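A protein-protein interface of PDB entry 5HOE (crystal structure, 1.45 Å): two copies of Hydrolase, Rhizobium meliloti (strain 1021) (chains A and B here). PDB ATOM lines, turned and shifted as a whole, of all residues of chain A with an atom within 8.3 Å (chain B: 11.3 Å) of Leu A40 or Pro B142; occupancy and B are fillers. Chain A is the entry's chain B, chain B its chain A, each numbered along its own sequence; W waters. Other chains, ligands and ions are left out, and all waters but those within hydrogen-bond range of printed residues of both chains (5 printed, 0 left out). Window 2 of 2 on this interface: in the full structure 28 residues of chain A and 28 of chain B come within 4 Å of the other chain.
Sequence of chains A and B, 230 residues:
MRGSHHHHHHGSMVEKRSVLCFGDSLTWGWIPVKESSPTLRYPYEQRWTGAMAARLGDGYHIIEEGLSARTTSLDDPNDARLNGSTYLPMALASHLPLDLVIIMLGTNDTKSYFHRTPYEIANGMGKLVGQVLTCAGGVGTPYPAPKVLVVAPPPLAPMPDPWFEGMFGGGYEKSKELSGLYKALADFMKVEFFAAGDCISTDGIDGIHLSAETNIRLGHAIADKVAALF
The backbone carbonyl oxygen of Leu B96 sits at hydrogen-bond distance from the indole nitrogen of Trp A28, at 3.1 Å.
O of Leu B96 lies within hydrogen-bond range of NH1 of Arg A41 (3.1 Å).
The backbone carbonyl oxygen (O) of Gly B140 sits at hydrogen-bond distance from the backbone NH (N) of Thr A39, at 3.0 Å.
The side-chain hydroxyl of Tyr B143 sits at hydrogen-bond distance from the backbone NH of Arg A41, at 2.9 Å.
OG1 of Thr B141 sits at hydrogen-bond distance from O of Gly B137 (2.7 Å).
The backbone NH (N) of Gly B137 sits at hydrogen-bond distance from the backbone carbonyl oxygen (O) of Tyr B143 (3.1 Å).
The side-chain hydroxyl (OG1) of Thr B141 sits at hydrogen-bond distance from the backbone NH (N) of Tyr B143 (3.1 Å).
The backbone NH (N) of Trp A30 sits at hydrogen-bond distance from the backbone carbonyl oxygen (O) of Ser A25 (3.1 Å).
The backbone carbonyl oxygen (O) of Trp A28 sits at hydrogen-bond distance from the guanidinium group (NE) of Arg A41.
The backbone carbonyl oxygen of Ile A31 sits at hydrogen-bond distance from the side-chain hydroxyl of Thr A39, at 2.7 Å.
Ala B93 touches Trp A28.
CD1 of Trp A28 touches O of Ser B94 (3.2 Å).
Trp A30 touches Val B139 (CZ3 to O, 3.7 Å).
CH2 of Trp A30 touches O of Gly B140, at 3.7 Å.
Thr B141 touches Thr A39.
Pro B142 touches Thr A39.
Leu A40 touches Pro B142.
Arg A41 touches His B95 (NH1 to O, 3.6 Å).
CD of Pro B97 touches CD of Arg A41 (3.9 Å).
Ser A68 touches Val B139.
Leu A40 touches just these residues of chain B: Pro B142 and Tyr B143.
Printed residues of chain A within 4 Å of Pro B142: Thr A39 and Leu A40.
No residue of chain B comes within 4 Å of Gly A29.
Trp A30 touches two residues of chain B.
No residue of chain B comes within 4 Å of Ile A31.
Printed residues of chain B within 4 Å of Thr A39: Gly B140 (3.0 Å), Thr B141 (3.5 Å) and Pro B142 (3.2 Å).
Of the printed residues of chain B, Pro A38 touches Gly B140 (3.2 Å) and Thr B141 (3.7 Å).
Of the printed residues of chain A, Tyr B143 touches Leu A40 and Arg A41.
Printed residues of chain A within 4 Å of Gly B140: Trp A30 (3.7 Å), Pro A38 (3.2 Å) and Thr A39 (3.0 Å).
Printed residues of chain A within 4 Å of His B95: Arg A41 (3.6 Å).
Printed residues of chain A within 4 Å of Ala B93: Trp A28.
Pro A43 touches none of the printed residues of chain B.
The nearest printed residue of chain A that does not touch Pro B142 is Pro A38 (4.01 Å).
The nearest printed residue of chain A that does not touch Thr B141 is Trp A30 (5.4 Å).
Of the 19 printed residues of chain B, 10 touch a printed residue of chain A.
Hydrophobic or aromatic side chains of chain B within 4 Å of the printed part of chain A: Pro B97, Val B139, Pro B142 and Tyr B143.
Of the 16 printed residues of chain A, 7 touch a printed residue of chain B.
Hydrophobic or aromatic side chains of chain A that line the printed part of chain B: Trp A28, Trp A30, Pro A38 and Leu A40.
Among the printed residues, 19 pairs touch across the chains.
Among the printed residues, no Asp or Glu carboxylate lies within 4 Å of a Lys or Arg side-chain nitrogen of the other chain.
No position is printed for both chains.
Water W1 bridges the backbone carbonyl oxygen (O) of Val B139 (2.6 Å) and the side-chain hydroxyl (OG) of Ser A68 (2.8 Å).
Water W4 lies within hydrogen-bond range of O of Ala B93 (2.8 Å) and N of Ser A68 (2.9 Å).
Water W5 lies within hydrogen-bond range of O of His B95 (2.8 Å), O of Pro B97 (2.9 Å) and NH1 of Arg A41 (3.5 Å).
Water W2 bridges the backbone carbonyl oxygen (O) of Ser B94 (2.9 Å) and the guanidinium group (NH2) of Arg A41 (3.4 Å).
Water W3 bridges ND1 of His B95 (2.9 Å) and NH1 of Arg A41 (3.2 Å).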
ATOM      1  N   SER A  25      -2.408  36.825 -21.185  1.00  0.00           N
ATOM      2  CA  SER A  25      -2.058  35.407 -21.341  1.00  0.00           C
ATOM      3  C   SER A  25      -1.270  35.146 -22.616  1.00  0.00           C
ATOM      4  O   SER A  25      -0.561  34.136 -22.705  1.00  0.00           O
ATOM      5  CB  SER A  25      -3.306  34.527 -21.378  1.00  0.00           C
ATOM      6  OG  SER A  25      -3.717  34.131 -20.083  1.00  0.00           O
ATOM      7  N   TRP A  28       2.159  35.881 -21.167  1.00  0.00           N
ATOM      8  CA  TRP A  28       2.490  34.898 -20.131  1.00  0.00           C
ATOM      9  C   TRP A  28       2.740  33.525 -20.734  1.00  0.00           C
ATOM     10  O   TRP A  28       3.658  32.806 -20.310  1.00  0.00           O
ATOM     11  CB  TRP A  28       1.357  34.823 -19.105  1.00  0.00           C
ATOM     12  CG  TRP A  28       1.612  33.818 -17.971  1.00  0.00           C
ATOM     13  CD1 TRP A  28       2.410  34.011 -16.883  1.00  0.00           C
ATOM     14  CD2 TRP A  28       1.044  32.508 -17.821  1.00  0.00           C
ATOM     15  NE1 TRP A  28       2.385  32.910 -16.077  1.00  0.00           N
ATOM     16  CE2 TRP A  28       1.550  31.973 -16.625  1.00  0.00           C
ATOM     17  CE3 TRP A  28       0.159  31.737 -18.583  1.00  0.00           C
ATOM     18  CZ2 TRP A  28       1.220  30.685 -16.183  1.00  0.00           C
ATOM     19  CZ3 TRP A  28      -0.181  30.482 -18.141  1.00  0.00           C
ATOM     20  CH2 TRP A  28       0.349  29.961 -16.950  1.00  0.00           C
ATOM     21  N   GLY A  29       1.957  33.158 -21.751  1.00  0.00           N
ATOM     22  CA  GLY A  29       2.143  31.888 -22.425  1.00  0.00           C
ATOM     23  C   GLY A  29       1.143  30.821 -22.037  1.00  0.00           C
ATOM     24  O   GLY A  29       1.538  29.710 -21.676  1.00  0.00           O
ATOM     25  N   TRP A  30      -0.150  31.146 -22.115  1.00  0.00           N
ATOM     26  CA  TRP A  30      -1.211  30.190 -21.823  1.00  0.00           C
ATOM     27  C   TRP A  30      -1.290  29.118 -22.926  1.00  0.00           C
ATOM     28  O   TRP A  30      -1.521  29.435 -24.094  1.00  0.00           O
ATOM     29  CB  TRP A  30      -2.526  30.969 -21.714  1.00  0.00           C
ATOM     30  CG  TRP A  30      -3.753  30.160 -21.454  1.00  0.00           C
ATOM     31  CD1 TRP A  30      -4.343  29.260 -22.297  1.00  0.00           C
ATOM     32  CD2 TRP A  30      -4.565  30.190 -20.269  1.00  0.00           C
ATOM     33  NE1 TRP A  30      -5.461  28.717 -21.701  1.00  0.00           N
ATOM     34  CE2 TRP A  30      -5.626  29.279 -20.463  1.00  0.00           C
ATOM     35  CE3 TRP A  30      -4.499  30.900 -19.068  1.00  0.00           C
ATOM     36  CZ2 TRP A  30      -6.603  29.052 -19.499  1.00  0.00           C
ATOM     37  CZ3 TRP A  30      -5.475  30.673 -18.103  1.00  0.00           C
ATOM     38  CH2 TRP A  30      -6.506  29.750 -18.322  1.00  0.00           C
ATOM     39  N   ILE A  31      -1.125  27.852 -22.558  1.00  0.00           N
ATOM     40  CA  ILE A  31      -1.256  26.744 -23.504  1.00  0.00           C
ATOM     41  C   ILE A  31      -2.732  26.435 -23.767  1.00  0.00           C
ATOM     42  O   ILE A  31      -3.454  26.037 -22.845  1.00  0.00           O
ATOM     43  CB  ILE A  31      -0.511  25.494 -23.008  1.00  0.00           C
ATOM     44  CG1 ILE A  31       0.960  25.823 -22.801  1.00  0.00           C
ATOM     45  CG2 ILE A  31      -0.674  24.351 -24.054  1.00  0.00           C
ATOM     46  CD1 ILE A  31       1.794  24.689 -22.217  1.00  0.00           C
ATOM     47  N   PRO A  32      -3.249  26.629 -24.982  1.00  0.00           N
ATOM     48  CA  PRO A  32      -4.652  26.272 -25.220  1.00  0.00           C
ATOM     49  C   PRO A  32      -4.851  24.778 -25.023  1.00  0.00           C
ATOM     50  O   PRO A  32      -4.051  23.965 -25.495  1.00  0.00           O
ATOM     51  CB  PRO A  32      -4.903  26.703 -26.672  1.00  0.00           C
ATOM     52  CG  PRO A  32      -3.578  26.998 -27.275  1.00  0.00           C
ATOM     53  CD  PRO A  32      -2.549  27.076 -26.198  1.00  0.00           C
ATOM     54  N   VAL A  33      -5.911  24.412 -24.291  1.00  0.00           N
ATOM     55  CA  VAL A  33      -6.213  23.008 -24.018  1.00  0.00           C
ATOM     56  C   VAL A  33      -7.702  22.715 -24.169  1.00  0.00           C
ATOM     57  O   VAL A  33      -8.559  23.580 -23.980  1.00  0.00           O
ATOM     58  CB  VAL A  33      -5.719  22.544 -22.630  1.00  0.00           C
ATOM     59  CG1 VAL A  33      -4.206  22.426 -22.619  1.00  0.00           C
ATOM     60  CG2 VAL A  33      -6.221  23.474 -21.544  1.00  0.00           C
ATOM     61  N   SER A  36     -10.232  23.711 -21.613  1.00  0.00           N
ATOM     62  CA  SER A  36     -10.262  25.170 -21.485  1.00  0.00           C
ATOM     63  C   SER A  36      -9.404  25.707 -20.344  1.00  0.00           C
ATOM     64  O   SER A  36      -8.575  26.591 -20.567  1.00  0.00           O
ATOM     65  CB  SER A  36     -11.689  25.707 -21.349  1.00  0.00           C
ATOM     66  OG  SER A  36     -12.433  25.511 -22.545  1.00  0.00           O
ATOM     67  N   SER A  37      -9.594  25.190 -19.134  1.00  0.00           N
ATOM     68  CA  SER A  37      -8.928  25.699 -17.938  1.00  0.00           C
ATOM     69  C   SER A  37      -9.015  24.617 -16.854  1.00  0.00           C
ATOM     70  O   SER A  37      -9.994  23.876 -16.806  1.00  0.00           O
ATOM     71  CB  SER A  37      -9.621  26.992 -17.457  1.00  0.00           C
ATOM     72  OG  SER A  37      -9.037  27.529 -16.268  1.00  0.00           O
ATOM     73  N   PRO A  38      -8.007  24.518 -15.968  1.00  0.00           N
ATOM     74  CA  PRO A  38      -6.754  25.280 -15.934  1.00  0.00           C
ATOM     75  C   PRO A  38      -5.736  24.748 -16.945  1.00  0.00           C
ATOM     76  O   PRO A  38      -5.994  23.748 -17.637  1.00  0.00           O
ATOM     77  CB  PRO A  38      -6.261  25.070 -14.496  1.00  0.00           C
ATOM     78  CG  PRO A  38      -6.714  23.696 -14.178  1.00  0.00           C
ATOM     79  CD  PRO A  38      -8.062  23.527 -14.876  1.00  0.00           C
ATOM     80  N   THR A  39      -4.594  25.420 -17.043  1.00  0.00           N
ATOM     81  CA  THR A  39      -3.586  25.035 -18.017  1.00  0.00           C
ATOM     82  C   THR A  39      -2.192  25.364 -17.501  1.00  0.00           C
ATOM     83  O   THR A  39      -2.007  26.100 -16.522  1.00  0.00           O
ATOM     84  CB  THR A  39      -3.820  25.698 -19.384  1.00  0.00           C
ATOM     85  OG1 THR A  39      -3.091  24.980 -20.390  1.00  0.00           O
ATOM     86  CG2 THR A  39      -3.355  27.144 -19.370  1.00  0.00           C
ATOM     87  N   LEU A  40      -1.213  24.855 -18.230  1.00  0.00           N
ATOM     88  CA  LEU A  40       0.197  25.055 -17.942  1.00  0.00           C
ATOM     89  C   LEU A  40       0.749  26.210 -18.770  1.00  0.00           C
ATOM     90  O   LEU A  40       0.112  26.713 -19.705  1.00  0.00           O
ATOM     91  CB  LEU A  40       0.971  23.774 -18.257  1.00  0.00           C
ATOM     92  CG  LEU A  40       0.535  22.571 -17.412  1.00  0.00           C
ATOM     93  CD1 LEU A  40       0.944  21.247 -18.052  1.00  0.00           C
ATOM     94  CD2 LEU A  40       1.111  22.684 -16.016  1.00  0.00           C
ATOM     95  N   ARG A  41       1.958  26.622 -18.423  1.00  0.00           N
ATOM     96  CA  ARG A  41       2.641  27.703 -19.117  1.00  0.00           C
ATOM     97  C   ARG A  41       3.617  27.148 -20.154  1.00  0.00           C
ATOM     98  O   ARG A  41       4.372  26.205 -19.879  1.00  0.00           O
ATOM     99  CB  ARG A  41       3.408  28.554 -18.104  1.00  0.00           C
ATOM    100  CG  ARG A  41       3.895  29.888 -18.631  1.00  0.00           C
ATOM    101  CD  ARG A  41       4.692  30.644 -17.565  1.00  0.00           C
ATOM    102  NE  ARG A  41       5.012  32.002 -17.987  1.00  0.00           N
ATOM    103  CZ  ARG A  41       5.749  32.849 -17.284  1.00  0.00           C
ATOM    104  NH1 ARG A  41       6.222  32.504 -16.090  1.00  0.00           N
ATOM    105  NH2 ARG A  41       6.005  34.048 -17.762  1.00  0.00           N
ATOM    106  N   TYR A  42       3.610  27.741 -21.351  1.00  0.00           N
ATOM    107  CA  TYR A  42       4.653  27.430 -22.316  1.00  0.00           C
ATOM    108  C   TYR A  42       6.026  27.671 -21.691  1.00  0.00           C
ATOM    109  O   TYR A  42       6.238  28.709 -21.041  1.00  0.00           O
ATOM    110  CB  TYR A  42       4.560  28.324 -23.559  1.00  0.00           C
ATOM    111  CG  TYR A  42       3.493  27.948 -24.545  1.00  0.00           C
ATOM    112  CD1 TYR A  42       3.566  26.747 -25.234  1.00  0.00           C
ATOM    113  CD2 TYR A  42       2.430  28.799 -24.799  1.00  0.00           C
ATOM    114  CE1 TYR A  42       2.601  26.387 -26.140  1.00  0.00           C
ATOM    115  CE2 TYR A  42       1.451  28.458 -25.713  1.00  0.00           C
ATOM    116  CZ  TYR A  42       1.538  27.240 -26.380  1.00  0.00           C
ATOM    117  OH  TYR A  42       0.610  26.831 -27.307  1.00  0.00           O
ATOM    118  N   PRO A  43       6.998  26.797 -21.944  1.00  0.00           N
ATOM    119  CA  PRO A  43       8.394  27.140 -21.654  1.00  0.00           C
ATOM    120  C   PRO A  43       8.829  28.412 -22.377  1.00  0.00           C
ATOM    121  O   PRO A  43       8.294  28.789 -23.421  1.00  0.00           O
ATOM    122  CB  PRO A  43       9.171  25.922 -22.184  1.00  0.00           C
ATOM    123  CG  PRO A  43       8.203  24.799 -22.117  1.00  0.00           C
ATOM    124  CD  PRO A  43       6.884  25.431 -22.496  1.00  0.00           C
ATOM    125  N   SER A  68      -2.167  36.589 -17.139  1.00  0.00           N
ATOM    126  CA  SER A  68      -3.422  36.099 -17.685  1.00  0.00           C
ATOM    127  C   SER A  68      -4.577  36.971 -17.202  1.00  0.00           C
ATOM    128  O   SER A  68      -4.664  37.331 -16.027  1.00  0.00           O
ATOM    129  CB  SER A  68      -3.638  34.648 -17.248  1.00  0.00           C
ATOM    130  OG  SER A  68      -2.653  33.807 -17.815  1.00  0.00           O
ATOM    131  N   ALA B  93       1.166  36.107  -9.718  1.00  0.00           N
ATOM    132  CA  ALA B  93       0.342  35.503 -10.757  1.00  0.00           C
ATOM    133  C   ALA B  93       0.996  35.653 -12.117  1.00  0.00           C
ATOM    134  O   ALA B  93       0.824  34.792 -12.988  1.00  0.00           O
ATOM    135  CB  ALA B  93      -1.061  36.119 -10.734  1.00  0.00           C
ATOM    136  N   SER B  94       1.764  36.722 -12.300  1.00  0.00           N
ATOM    137  CA  SER B  94       2.478  36.959 -13.545  1.00  0.00           C
ATOM    138  C   SER B  94       3.659  36.017 -13.729  1.00  0.00           C
ATOM    139  O   SER B  94       4.119  35.835 -14.862  1.00  0.00           O
ATOM    140  CB  SER B  94       3.010  38.386 -13.585  1.00  0.00           C
ATOM    141  OG  SER B  94       2.000  39.357 -13.495  1.00  0.00           O
ATOM    142  N   HIS B  95       4.204  35.468 -12.648  1.00  0.00           N
ATOM    143  CA  HIS B  95       5.450  34.713 -12.732  1.00  0.00           C
ATOM    144  C   HIS B  95       5.326  33.240 -12.391  1.00  0.00           C
ATOM    145  O   HIS B  95       6.332  32.537 -12.460  1.00  0.00           O
ATOM    146  CB  HIS B  95       6.537  35.399 -11.896  1.00  0.00           C
ATOM    147  CG  HIS B  95       6.881  36.753 -12.418  1.00  0.00           C
ATOM    148  ND1 HIS B  95       7.323  36.961 -13.706  1.00  0.00           N
ATOM    149  CD2 HIS B  95       6.784  37.976 -11.851  1.00  0.00           C
ATOM    150  CE1 HIS B  95       7.500  38.255 -13.903  1.00  0.00           C
ATOM    151  NE2 HIS B  95       7.178  38.892 -12.791  1.00  0.00           N
ATOM    152  N   LEU B  96       4.124  32.733 -12.123  1.00  0.00           N
ATOM    153  CA  LEU B  96       3.961  31.291 -11.920  1.00  0.00           C
ATOM    154  C   LEU B  96       4.353  30.575 -13.211  1.00  0.00           C
ATOM    155  O   LEU B  96       4.176  31.114 -14.299  1.00  0.00           O
ATOM    156  CB  LEU B  96       2.534  30.946 -11.512  1.00  0.00           C
ATOM    157  CG  LEU B  96       2.072  31.349 -10.107  1.00  0.00           C
ATOM    158  CD1 LEU B  96       0.674  30.818  -9.838  1.00  0.00           C
ATOM    159  CD2 LEU B  96       3.013  30.860  -9.012  1.00  0.00           C
ATOM    160  N   PRO B  97       4.909  29.360 -13.103  1.00  0.00           N
ATOM    161  CA  PRO B  97       5.177  28.595 -11.882  1.00  0.00           C
ATOM    162  C   PRO B  97       6.410  29.097 -11.130  1.00  0.00           C
ATOM    163  O   PRO B  97       7.411  29.452 -11.768  1.00  0.00           O
ATOM    164  CB  PRO B  97       5.421  27.184 -12.434  1.00  0.00           C
ATOM    165  CG  PRO B  97       6.063  27.423 -13.743  1.00  0.00           C
ATOM    166  CD  PRO B  97       5.283  28.594 -14.307  1.00  0.00           C
ATOM    167  N   LEU B  98       6.332  29.138  -9.798  1.00  0.00           N
ATOM    168  CA  LEU B  98       7.426  29.596  -8.951  1.00  0.00           C
ATOM    169  C   LEU B  98       7.722  28.536  -7.907  1.00  0.00           C
ATOM    170  O   LEU B  98       6.801  28.019  -7.268  1.00  0.00           O
ATOM    171  CB  LEU B  98       7.074  30.910  -8.239  1.00  0.00           C
ATOM    172  CG  LEU B  98       6.972  32.178  -9.093  1.00  0.00           C
ATOM    173  CD1 LEU B  98       6.470  33.296  -8.220  1.00  0.00           C
ATOM    174  CD2 LEU B  98       8.326  32.541  -9.712  1.00  0.00           C
ATOM    175  N   THR B 134      -0.846  31.772  -0.130  1.00  0.00           N
ATOM    176  CA  THR B 134      -2.213  31.603  -0.600  1.00  0.00           C
ATOM    177  C   THR B 134      -2.348  31.778  -2.106  1.00  0.00           C
ATOM    178  O   THR B 134      -3.478  31.816  -2.604  1.00  0.00           O
ATOM    179  CB  THR B 134      -3.172  32.556   0.123  1.00  0.00           C
ATOM    180  OG1 THR B 134      -2.841  33.917  -0.185  1.00  0.00           O
ATOM    181  CG2 THR B 134      -3.113  32.347   1.634  1.00  0.00           C
ATOM    182  N   CYS B 135      -1.233  31.866  -2.848  1.00  0.00           N
ATOM    183  CA  CYS B 135      -1.283  32.246  -4.257  1.00  0.00           C
ATOM    184  C   CYS B 135      -1.467  31.072  -5.215  1.00  0.00           C
ATOM    185  O   CYS B 135      -1.486  31.292  -6.434  1.00  0.00           O
ATOM    186  CB  CYS B 135      -0.031  33.046  -4.654  1.00  0.00           C
ATOM    187  SG  CYS B 135       1.454  32.074  -5.048  1.00  0.00           S
ATOM    188  N   ALA B 136      -1.628  29.855  -4.706  1.00  0.00           N
ATOM    189  CA  ALA B 136      -1.728  28.682  -5.565  1.00  0.00           C
ATOM    190  C   ALA B 136      -2.796  28.895  -6.621  1.00  0.00           C
ATOM    191  O   ALA B 136      -3.875  29.424  -6.339  1.00  0.00           O
ATOM    192  CB  ALA B 136      -2.077  27.440  -4.733  1.00  0.00           C
ATOM    193  N   GLY B 137      -2.483  28.478  -7.846  1.00  0.00           N
ATOM    194  CA  GLY B 137      -3.416  28.601  -8.948  1.00  0.00           C
ATOM    195  C   GLY B 137      -3.135  29.800  -9.825  1.00  0.00           C
ATOM    196  O   GLY B 137      -3.273  29.719 -11.047  1.00  0.00           O
ATOM    197  N   GLY B 138      -2.732  30.914  -9.224  1.00  0.00           N
ATOM    198  CA  GLY B 138      -2.636  32.150  -9.991  1.00  0.00           C
ATOM    199  C   GLY B 138      -3.949  32.432 -10.686  1.00  0.00           C
ATOM    200  O   GLY B 138      -5.024  32.343 -10.083  1.00  0.00           O
ATOM    201  N   VAL B 139      -3.864  32.774 -11.969  1.00  0.00           N
ATOM    202  CA  VAL B 139      -5.023  32.917 -12.843  1.00  0.00           C
ATOM    203  C   VAL B 139      -5.068  31.659 -13.708  1.00  0.00           C
ATOM    204  O   VAL B 139      -4.338  31.552 -14.692  1.00  0.00           O
ATOM    205  CB  VAL B 139      -4.921  34.169 -13.722  1.00  0.00           C
ATOM    206  CG1 VAL B 139      -6.165  34.296 -14.610  1.00  0.00           C
ATOM    207  CG2 VAL B 139      -4.733  35.431 -12.913  1.00  0.00           C
ATOM    208  N   GLY B 140      -5.906  30.692 -13.329  1.00  0.00           N
ATOM    209  CA  GLY B 140      -6.218  29.554 -14.187  1.00  0.00           C
ATOM    210  C   GLY B 140      -5.124  28.517 -14.384  1.00  0.00           C
ATOM    211  O   GLY B 140      -5.038  27.927 -15.470  1.00  0.00           O
ATOM    212  N   THR B 141      -4.300  28.255 -13.372  1.00  0.00           N
ATOM    213  CA  THR B 141      -3.260  27.241 -13.468  1.00  0.00           C
ATOM    214  C   THR B 141      -3.406  26.196 -12.370  1.00  0.00           C
ATOM    215  O   THR B 141      -4.096  26.418 -11.368  1.00  0.00           O
ATOM    216  CB  THR B 141      -1.849  27.841 -13.358  1.00  0.00           C
ATOM    217  OG1 THR B 141      -1.470  27.940 -11.972  1.00  0.00           O
ATOM    218  CG2 THR B 141      -1.768  29.211 -14.024  1.00  0.00           C
ATOM    219  N   PRO B 142      -2.764  25.041 -12.525  1.00  0.00           N
ATOM    220  CA  PRO B 142      -2.724  24.043 -11.449  1.00  0.00           C
ATOM    221  C   PRO B 142      -1.488  24.142 -10.570  1.00  0.00           C
ATOM    222  O   PRO B 142      -1.237  23.219  -9.796  1.00  0.00           O
ATOM    223  CB  PRO B 142      -2.673  22.741 -12.253  1.00  0.00           C
ATOM    224  CG  PRO B 142      -1.768  23.102 -13.405  1.00  0.00           C
ATOM    225  CD  PRO B 142      -2.061  24.554 -13.728  1.00  0.00           C
ATOM    226  N   TYR B 143      -0.717  25.218 -10.676  1.00  0.00           N
ATOM    227  CA  TYR B 143       0.585  25.258 -10.034  1.00  0.00           C
ATOM    228  C   TYR B 143       0.447  25.453  -8.520  1.00  0.00           C
ATOM    229  O   TYR B 143      -0.462  26.145  -8.054  1.00  0.00           O
ATOM    230  CB  TYR B 143       1.401  26.401 -10.625  1.00  0.00           C
ATOM    231  CG  TYR B 143       1.852  26.165 -12.056  1.00  0.00           C
ATOM    232  CD1 TYR B 143       2.515  24.993 -12.417  1.00  0.00           C
ATOM    233  CD2 TYR B 143       1.614  27.116 -13.041  1.00  0.00           C
ATOM    234  CE1 TYR B 143       2.949  24.785 -13.713  1.00  0.00           C
ATOM    235  CE2 TYR B 143       2.033  26.913 -14.349  1.00  0.00           C
ATOM    236  CZ  TYR B 143       2.694  25.747 -14.682  1.00  0.00           C
ATOM    237  OH  TYR B 143       3.130  25.557 -15.974  1.00  0.00           O
ATOM    238  N   PRO B 144       1.345  24.864  -7.734  1.00  0.00           N
ATOM    239  CA  PRO B 144       1.264  24.986  -6.273  1.00  0.00           C
ATOM    240  C   PRO B 144       1.844  26.301  -5.768  1.00  0.00           C
ATOM    241  O   PRO B 144       2.530  27.037  -6.477  1.00  0.00           O
ATOM    242  CB  PRO B 144       2.135  23.824  -5.782  1.00  0.00           C
ATOM    243  CG  PRO B 144       3.160  23.679  -6.849  1.00  0.00           C
ATOM    244  CD  PRO B 144       2.405  23.927  -8.140  1.00  0.00           C
ATOM    245  N   ALA B 145       1.571  26.568  -4.500  1.00  0.00           N
ATOM    246  CA  ALA B 145       2.188  27.711  -3.854  1.00  0.00           C
ATOM    247  C   ALA B 145       3.705  27.521  -3.753  1.00  0.00           C
ATOM    248  O   ALA B 145       4.186  26.412  -3.459  1.00  0.00           O
ATOM    249  CB  ALA B 145       1.611  27.930  -2.458  1.00  0.00           C
ATOM    250  N   PRO B 146       4.479  28.583  -3.979  1.00  0.00           N
ATOM    251  CA  PRO B 146       5.929  28.527  -3.777  1.00  0.00           C
ATOM    252  C   PRO B 146       6.281  28.423  -2.305  1.00  0.00           C
ATOM    253  O   PRO B 146       5.483  28.751  -1.425  1.00  0.00           O
ATOM    254  CB  PRO B 146       6.409  29.890  -4.304  1.00  0.00           C
ATOM    255  CG  PRO B 146       5.252  30.546  -4.929  1.00  0.00           C
ATOM    256  CD  PRO B 146       4.033  29.925  -4.386  1.00  0.00           C
HETATM  257  O   HOH W   1      -2.016  32.066 -15.755  1.00  0.00           O
HETATM  258  O   HOH W   2       5.415  37.324 -16.963  1.00  0.00           O
HETATM  259  O   HOH W   3       8.215  34.879 -15.497  1.00  0.00           O
HETATM  260  O   HOH W   4      -0.499  34.907 -15.443  1.00  0.00           O
HETATM  261  O   HOH W   5       8.501  31.292 -13.758  1.00  0.00           O
